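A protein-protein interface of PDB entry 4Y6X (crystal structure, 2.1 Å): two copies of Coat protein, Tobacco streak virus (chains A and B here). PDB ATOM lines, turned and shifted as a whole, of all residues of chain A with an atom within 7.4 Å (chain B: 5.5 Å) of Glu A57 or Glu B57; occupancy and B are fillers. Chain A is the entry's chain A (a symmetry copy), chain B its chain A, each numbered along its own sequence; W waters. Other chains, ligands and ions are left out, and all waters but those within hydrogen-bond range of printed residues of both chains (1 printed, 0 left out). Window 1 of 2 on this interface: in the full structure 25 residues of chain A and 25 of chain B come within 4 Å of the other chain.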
ATOM      1  N   VAL A  26      -4.451 -28.643  -1.783  1.00  0.00           N
ATOM      2  CA  VAL A  26      -5.640 -28.617  -0.957  1.00  0.00           C
ATOM      3  C   VAL A  26      -6.449 -27.339  -1.231  1.00  0.00           C
ATOM      4  O   VAL A  26      -5.934 -26.352  -1.760  1.00  0.00           O
ATOM      5  CB  VAL A  26      -5.336 -28.652   0.557  1.00  0.00           C
ATOM      6  CG1 VAL A  26      -4.750 -29.997   0.930  1.00  0.00           C
ATOM      7  CG2 VAL A  26      -4.405 -27.514   0.969  1.00  0.00           C
ATOM      8  N   TRP A  27      -7.703 -27.393  -0.823  1.00  0.00           N
ATOM      9  CA  TRP A  27      -8.610 -26.264  -0.796  1.00  0.00           C
ATOM     10  C   TRP A  27      -8.482 -25.566   0.513  1.00  0.00           C
ATOM     11  O   TRP A  27      -8.439 -26.223   1.551  1.00  0.00           O
ATOM     12  CB  TRP A  27     -10.057 -26.709  -0.959  1.00  0.00           C
ATOM     13  CG  TRP A  27     -10.429 -27.165  -2.352  1.00  0.00           C
ATOM     14  CD1 TRP A  27     -10.724 -28.432  -2.755  1.00  0.00           C
ATOM     15  CD2 TRP A  27     -10.520 -26.342  -3.508  1.00  0.00           C
ATOM     16  NE1 TRP A  27     -11.044 -28.429  -4.096  1.00  0.00           N
ATOM     17  CE2 TRP A  27     -10.885 -27.169  -4.587  1.00  0.00           C
ATOM     18  CE3 TRP A  27     -10.398 -24.962  -3.724  1.00  0.00           C
ATOM     19  CZ2 TRP A  27     -11.085 -26.685  -5.841  1.00  0.00           C
ATOM     20  CZ3 TRP A  27     -10.553 -24.488  -4.973  1.00  0.00           C
ATOM     21  CH2 TRP A  27     -10.927 -25.325  -6.023  1.00  0.00           C
ATOM     22  N   VAL A  28      -8.417 -24.246   0.464  1.00  0.00           N
ATOM     23  CA  VAL A  28      -8.628 -23.433   1.621  1.00  0.00           C
ATOM     24  C   VAL A  28      -9.670 -22.397   1.278  1.00  0.00           C
ATOM     25  O   VAL A  28      -9.950 -22.133   0.076  1.00  0.00           O
ATOM     26  CB  VAL A  28      -7.319 -22.744   2.086  1.00  0.00           C
ATOM     27  CG1 VAL A  28      -6.278 -23.805   2.527  1.00  0.00           C
ATOM     28  CG2 VAL A  28      -6.755 -21.835   1.028  1.00  0.00           C
ATOM     29  N   THR A  29     -10.301 -21.806   2.298  1.00  0.00           N
ATOM     30  CA  THR A  29     -11.397 -20.891   2.060  1.00  0.00           C
ATOM     31  C   THR A  29     -11.390 -19.842   3.114  1.00  0.00           C
ATOM     32  O   THR A  29     -10.874 -20.084   4.207  1.00  0.00           O
ATOM     33  CB  THR A  29     -12.788 -21.591   2.084  1.00  0.00           C
ATOM     34  OG1 THR A  29     -13.842 -20.664   1.740  1.00  0.00           O
ATOM     35  CG2 THR A  29     -13.147 -22.167   3.494  1.00  0.00           C
ATOM     36  N   GLY A  54      -5.599 -13.463   6.130  1.00  0.00           N
ATOM     37  CA  GLY A  54      -6.353 -14.218   7.135  1.00  0.00           C
ATOM     38  C   GLY A  54      -6.601 -15.674   6.759  1.00  0.00           C
ATOM     39  O   GLY A  54      -7.653 -16.228   7.101  1.00  0.00           O
ATOM     40  N   ILE A  55      -5.625 -16.298   6.081  1.00  0.00           N
ATOM     41  CA  ILE A  55      -5.640 -17.725   5.834  1.00  0.00           C
ATOM     42  C   ILE A  55      -4.316 -18.293   6.341  1.00  0.00           C
ATOM     43  O   ILE A  55      -3.273 -18.121   5.737  1.00  0.00           O
ATOM     44  CB  ILE A  55      -5.847 -18.055   4.358  1.00  0.00           C
ATOM     45  CG1 ILE A  55      -7.168 -17.451   3.871  1.00  0.00           C
ATOM     46  CG2 ILE A  55      -5.798 -19.560   4.148  1.00  0.00           C
ATOM     47  CD1 ILE A  55      -7.536 -17.787   2.434  1.00  0.00           C
ATOM     48  N   PRO A  56      -4.348 -18.990   7.475  1.00  0.00           N
ATOM     49  CA  PRO A  56      -3.077 -19.432   8.101  1.00  0.00           C
ATOM     50  C   PRO A  56      -2.196 -20.433   7.315  1.00  0.00           C
ATOM     51  O   PRO A  56      -0.990 -20.366   7.421  1.00  0.00           O
ATOM     52  CB  PRO A  56      -3.544 -20.044   9.439  1.00  0.00           C
ATOM     53  CG  PRO A  56      -4.985 -20.414   9.212  1.00  0.00           C
ATOM     54  CD  PRO A  56      -5.536 -19.379   8.259  1.00  0.00           C
ATOM     55  N   GLU A  57      -2.770 -21.322   6.514  1.00  0.00           N
ATOM     56  CA  GLU A  57      -1.994 -22.256   5.657  1.00  0.00           C
ATOM     57  C   GLU A  57      -1.086 -21.581   4.572  1.00  0.00           C
ATOM     58  O   GLU A  57      -0.387 -22.276   3.846  1.00  0.00           O
ATOM     59  CB  GLU A  57      -2.947 -23.201   4.889  1.00  0.00           C
ATOM     60  CG  GLU A  57      -3.725 -24.186   5.743  1.00  0.00           C
ATOM     61  CD  GLU A  57      -5.088 -23.679   6.229  1.00  0.00           C
ATOM     62  OE1 GLU A  57      -5.305 -22.428   6.340  1.00  0.00           O
ATOM     63  OE2 GLU A  57      -5.943 -24.550   6.532  1.00  0.00           O
ATOM     64  N   ILE A  58      -1.155 -20.261   4.437  1.00  0.00           N
ATOM     65  CA  ILE A  58      -0.528 -19.541   3.357  1.00  0.00           C
ATOM     66  C   ILE A  58       0.688 -18.729   3.815  1.00  0.00           C
ATOM     67  O   ILE A  58       0.622 -18.003   4.788  1.00  0.00           O
ATOM     68  CB  ILE A  58      -1.561 -18.592   2.684  1.00  0.00           C
ATOM     69  CG1 ILE A  58      -2.526 -19.448   1.841  1.00  0.00           C
ATOM     70  CG2 ILE A  58      -0.852 -17.566   1.824  1.00  0.00           C
ATOM     71  CD1 ILE A  58      -3.749 -18.737   1.328  1.00  0.00           C
ATOM     72  N   ASN A  59       1.774 -18.822   3.057  1.00  0.00           N
ATOM     73  CA  ASN A  59       3.002 -18.084   3.335  1.00  0.00           C
ATOM     74  C   ASN A  59       3.706 -17.756   2.021  1.00  0.00           C
ATOM     75  O   ASN A  59       3.125 -17.960   0.942  1.00  0.00           O
ATOM     76  CB  ASN A  59       3.907 -18.937   4.221  1.00  0.00           C
ATOM     77  CG  ASN A  59       4.260 -20.237   3.580  1.00  0.00           C
ATOM     78  OD1 ASN A  59       4.891 -20.275   2.526  1.00  0.00           O
ATOM     79  ND2 ASN A  59       3.798 -21.313   4.162  1.00  0.00           N
ATOM     80  N   THR A  62       3.925 -20.549  -0.661  1.00  0.00           N
ATOM     81  CA  THR A  62       2.728 -21.195  -1.183  1.00  0.00           C
ATOM     82  C   THR A  62       2.575 -20.953  -2.686  1.00  0.00           C
ATOM     83  O   THR A  62       2.661 -19.838  -3.117  1.00  0.00           O
ATOM     84  CB  THR A  62       1.483 -20.673  -0.460  1.00  0.00           C
ATOM     85  OG1 THR A  62       1.626 -20.940   0.941  1.00  0.00           O
ATOM     86  CG2 THR A  62       0.204 -21.397  -0.989  1.00  0.00           C
ATOM     87  N   ILE A 149      -4.300 -24.481  -3.227  1.00  0.00           N
ATOM     88  CA  ILE A 149      -2.931 -24.180  -2.963  1.00  0.00           C
ATOM     89  C   ILE A 149      -2.105 -25.453  -2.834  1.00  0.00           C
ATOM     90  O   ILE A 149      -2.639 -26.550  -2.634  1.00  0.00           O
ATOM     91  CB  ILE A 149      -2.772 -23.367  -1.707  1.00  0.00           C
ATOM     92  CG1 ILE A 149      -3.292 -24.127  -0.522  1.00  0.00           C
ATOM     93  CG2 ILE A 149      -3.481 -22.026  -1.864  1.00  0.00           C
ATOM     94  CD1 ILE A 149      -2.895 -23.516   0.806  1.00  0.00           C
ATOM     95  N   SER A 150      -0.808 -25.296  -2.899  1.00  0.00           N
ATOM     96  CA  SER A 150       0.120 -26.392  -2.557  1.00  0.00           C
ATOM     97  C   SER A 150      -0.134 -26.845  -1.136  1.00  0.00           C
ATOM     98  O   SER A 150      -0.358 -26.017  -0.233  1.00  0.00           O
ATOM     99  CB  SER A 150       1.613 -25.968  -2.742  1.00  0.00           C
ATOM    100  OG  SER A 150       1.886 -24.653  -2.287  1.00  0.00           O
ATOM    101  N   LYS A 151      -0.166 -28.155  -0.969  1.00  0.00           N
ATOM    102  CA  LYS A 151      -0.531 -28.779   0.298  1.00  0.00           C
ATOM    103  C   LYS A 151       0.514 -28.459   1.370  1.00  0.00           C
ATOM    104  O   LYS A 151       1.695 -28.658   1.157  1.00  0.00           O
ATOM    105  CB  LYS A 151      -0.620 -30.268   0.130  1.00  0.00           C
ATOM    106  CG  LYS A 151      -0.952 -31.042   1.374  1.00  0.00           C
ATOM    107  CD  LYS A 151      -1.180 -32.517   0.940  1.00  0.00           C
ATOM    108  CE  LYS A 151      -2.604 -32.719   0.470  1.00  0.00           C
ATOM    109  NZ  LYS A 151      -2.941 -34.155   0.282  1.00  0.00           N
ATOM    110  N   PRO A 152       0.078 -27.875   2.497  1.00  0.00           N
ATOM    111  CA  PRO A 152       1.008 -27.509   3.545  1.00  0.00           C
ATOM    112  C   PRO A 152       1.363 -28.708   4.421  1.00  0.00           C
ATOM    113  O   PRO A 152       0.658 -29.687   4.436  1.00  0.00           O
ATOM    114  CB  PRO A 152       0.208 -26.441   4.344  1.00  0.00           C
ATOM    115  CG  PRO A 152      -1.216 -26.840   4.198  1.00  0.00           C
ATOM    116  CD  PRO A 152      -1.321 -27.478   2.823  1.00  0.00           C
ATOM    117  N   ALA A 153       2.441 -28.622   5.186  1.00  0.00           N
ATOM    118  CA  ALA A 153       2.678 -29.603   6.270  1.00  0.00           C
ATOM    119  C   ALA A 153       1.510 -29.565   7.287  1.00  0.00           C
ATOM    120  O   ALA A 153       0.824 -28.564   7.398  1.00  0.00           O
ATOM    121  CB  ALA A 153       3.972 -29.261   6.990  1.00  0.00           C
ATOM    122  N   LEU A 155      -0.640 -28.734  10.334  1.00  0.00           N
ATOM    123  CA  LEU A 155      -0.566 -27.486  11.055  1.00  0.00           C
ATOM    124  C   LEU A 155      -0.192 -27.757  12.540  1.00  0.00           C
ATOM    125  O   LEU A 155      -0.712 -28.680  13.172  1.00  0.00           O
ATOM    126  CB  LEU A 155      -1.890 -26.801  10.874  1.00  0.00           C
ATOM    127  CG  LEU A 155      -1.984 -25.355  11.226  1.00  0.00           C
ATOM    128  CD1 LEU A 155      -1.002 -24.555  10.388  1.00  0.00           C
ATOM    129  CD2 LEU A 155      -3.412 -24.881  11.010  1.00  0.00           C
ATOM    130  N   VAL B  28      -6.148 -25.894  14.652  1.00  0.00           N
ATOM    131  CA  VAL B  28      -6.489 -24.793  13.805  1.00  0.00           C
ATOM    132  C   VAL B  28      -6.111 -23.521  14.523  1.00  0.00           C
ATOM    133  O   VAL B  28      -5.909 -23.515  15.769  1.00  0.00           O
ATOM    134  CB  VAL B  28      -7.999 -24.783  13.453  1.00  0.00           C
ATOM    135  CG1 VAL B  28      -8.371 -26.047  12.636  1.00  0.00           C
ATOM    136  CG2 VAL B  28      -8.862 -24.655  14.680  1.00  0.00           C
ATOM    137  N   ILE B  55     -13.121 -19.316  11.390  1.00  0.00           N
ATOM    138  CA  ILE B  55     -12.346 -20.527  11.210  1.00  0.00           C
ATOM    139  C   ILE B  55     -13.221 -21.522  10.449  1.00  0.00           C
ATOM    140  O   ILE B  55     -14.147 -22.101  10.987  1.00  0.00           O
ATOM    141  CB  ILE B  55     -11.876 -21.117  12.537  1.00  0.00           C
ATOM    142  CG1 ILE B  55     -11.024 -20.088  13.289  1.00  0.00           C
ATOM    143  CG2 ILE B  55     -11.118 -22.412  12.293  1.00  0.00           C
ATOM    144  CD1 ILE B  55     -10.416 -20.587  14.591  1.00  0.00           C
ATOM    145  N   PRO B  56     -12.928 -21.734   9.168  1.00  0.00           N
ATOM    146  CA  PRO B  56     -13.832 -22.565   8.335  1.00  0.00           C
ATOM    147  C   PRO B  56     -13.996 -24.056   8.717  1.00  0.00           C
ATOM    148  O   PRO B  56     -15.065 -24.597   8.535  1.00  0.00           O
ATOM    149  CB  PRO B  56     -13.230 -22.423   6.921  1.00  0.00           C
ATOM    150  CG  PRO B  56     -11.793 -22.039   7.151  1.00  0.00           C
ATOM    151  CD  PRO B  56     -11.781 -21.200   8.408  1.00  0.00           C
ATOM    152  N   GLU B  57     -12.979 -24.707   9.269  1.00  0.00           N
ATOM    153  CA  GLU B  57     -13.082 -26.111   9.747  1.00  0.00           C
ATOM    154  C   GLU B  57     -14.114 -26.357  10.901  1.00  0.00           C
ATOM    155  O   GLU B  57     -14.286 -27.490  11.331  1.00  0.00           O
ATOM    156  CB  GLU B  57     -11.716 -26.599  10.282  1.00  0.00           C
ATOM    157  CG  GLU B  57     -10.616 -26.737   9.246  1.00  0.00           C
ATOM    158  CD  GLU B  57      -9.761 -25.480   9.046  1.00  0.00           C
ATOM    159  OE1 GLU B  57     -10.234 -24.330   9.325  1.00  0.00           O
ATOM    160  OE2 GLU B  57      -8.606 -25.648   8.575  1.00  0.00           O
ATOM    161  N   ILE B  58     -14.729 -25.300  11.422  1.00  0.00           N
ATOM    162  CA  ILE B  58     -15.545 -25.363  12.608  1.00  0.00           C
ATOM    163  C   ILE B  58     -17.039 -25.208  12.307  1.00  0.00           C
ATOM    164  O   ILE B  58     -17.441 -24.306  11.598  1.00  0.00           O
ATOM    165  CB  ILE B  58     -15.102 -24.262  13.614  1.00  0.00           C
ATOM    166  CG1 ILE B  58     -13.766 -24.694  14.248  1.00  0.00           C
ATOM    167  CG2 ILE B  58     -16.165 -24.057  14.674  1.00  0.00           C
ATOM    168  CD1 ILE B  58     -13.051 -23.639  15.047  1.00  0.00           C
ATOM    169  N   ASN B  59     -17.851 -26.068  12.911  1.00  0.00           N
ATOM    170  CA  ASN B  59     -19.302 -26.031  12.758  1.00  0.00           C
ATOM    171  C   ASN B  59     -19.960 -26.517  14.047  1.00  0.00           C
ATOM    172  O   ASN B  59     -19.269 -26.695  15.064  1.00  0.00           O
ATOM    173  CB  ASN B  59     -19.703 -26.927  11.589  1.00  0.00           C
ATOM    174  CG  ASN B  59     -19.276 -28.341  11.789  1.00  0.00           C
ATOM    175  OD1 ASN B  59     -19.704 -29.007  12.730  1.00  0.00           O
ATOM    176  ND2 ASN B  59     -18.373 -28.796  10.960  1.00  0.00           N
ATOM    177  N   THR B  62     -18.472 -29.658  15.767  1.00  0.00           N
ATOM    178  CA  THR B  62     -17.074 -29.709  16.176  1.00  0.00           C
ATOM    179  C   THR B  62     -16.943 -29.874  17.691  1.00  0.00           C
ATOM    180  O   THR B  62     -17.558 -29.150  18.420  1.00  0.00           O
ATOM    181  CB  THR B  62     -16.347 -28.432  15.744  1.00  0.00           C
ATOM    182  OG1 THR B  62     -16.448 -28.310  14.320  1.00  0.00           O
ATOM    183  CG2 THR B  62     -14.839 -28.504  16.144  1.00  0.00           C
ATOM    184  N   ILE B 149      -9.218 -29.298  17.753  1.00  0.00           N
ATOM    185  CA  ILE B 149     -10.561 -29.690  17.474  1.00  0.00           C
ATOM    186  C   ILE B 149     -10.614 -31.104  16.910  1.00  0.00           C
ATOM    187  O   ILE B 149      -9.608 -31.649  16.443  1.00  0.00           O
ATOM    188  CB  ILE B 149     -11.224 -28.752  16.502  1.00  0.00           C
ATOM    189  CG1 ILE B 149     -10.487 -28.746  15.194  1.00  0.00           C
ATOM    190  CG2 ILE B 149     -11.304 -27.353  17.104  1.00  0.00           C
ATOM    191  CD1 ILE B 149     -11.254 -28.073  14.075  1.00  0.00           C
ATOM    192  N   PRO B 152     -11.663 -32.623  10.939  1.00  0.00           N
ATOM    193  CA  PRO B 152     -12.733 -32.505   9.970  1.00  0.00           C
ATOM    194  C   PRO B 152     -12.485 -33.396   8.755  1.00  0.00           C
ATOM    195  O   PRO B 152     -11.379 -33.812   8.514  1.00  0.00           O
ATOM    196  CB  PRO B 152     -12.673 -30.998   9.589  1.00  0.00           C
ATOM    197  CG  PRO B 152     -11.243 -30.623   9.731  1.00  0.00           C
ATOM    198  CD  PRO B 152     -10.707 -31.482  10.862  1.00  0.00           C
ATOM    199  N   LEU B 155     -11.266 -30.649   3.284  1.00  0.00           N
ATOM    200  CA  LEU B 155     -12.037 -29.474   2.955  1.00  0.00           C
ATOM    201  C   LEU B 155     -12.340 -29.451   1.430  1.00  0.00           C
ATOM    202  O   LEU B 155     -11.472 -29.738   0.601  1.00  0.00           O
ATOM    203  CB  LEU B 155     -11.252 -28.289   3.440  1.00  0.00           C
ATOM    204  CG  LEU B 155     -11.952 -26.976   3.535  1.00  0.00           C
ATOM    205  CD1 LEU B 155     -13.132 -27.088   4.485  1.00  0.00           C
ATOM    206  CD2 LEU B 155     -10.965 -25.917   3.999  1.00  0.00           C
HETATM  207  O   HOH W   1      -8.766 -29.848   0.556  1.00  0.00           O
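Trp A27 touches Leu B155 (O to CD2, 3.5 Å). Thr A29 touches Pro B56 (CG2 to CB, 3.4 Å). OE2 of Glu A57 touches OE2 of Glu B57, at 3.5 Å.
Of the printed residues of chain B, Trp A27 touches Leu B155 (3.5 Å). Of the printed residues of chain B, Thr A29 touches Pro B56. Ile A55 touches none of the printed residues of chain B. Glu A57 touches one residue of chain B. Ile A149 touches none of the printed residues of chain B. Printed residues of chain A within 4 Å of Pro B56: Thr A29. Printed residues of chain A within 4 Å of Glu B57: Glu A57. The nearest printed residue of chain B that does not touch Glu A57 is Leu B155 (5.8 Å). The nearest residue of chain A that does not touch Glu B57 is Leu A155 (5.8 Å). The nearest printed residue of chain A that does not touch Pro B56 is Val A28 (6.3 Å).
Hydrophobic or aromatic side chains of chain B within 4 Å of the printed part of chain A: Pro B56 and Leu B155. Printed residues of chain A that touch a printed residue of chain B: Trp A27, Thr A29 and Glu A57. Hydrophobic or aromatic side chains of chain A within 4 Å of the printed part of chain B: Trp A27. Among the printed residues, 3 pairs touch across the chains.
Glu A57 touches its own counterpart, Glu B57. Positions printed for both chains: 28, 55, 56, 57, 58, 59, 62, 149, 152 and 155. Of the 3 pairs that touch across the chains among the printed residues, 1 has its exchanged pair printed and touching as well.
Water W1 lies within hydrogen-bond range of O of Leu B155 (2.7 Å) and N of Trp A27 (3.0 Å).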
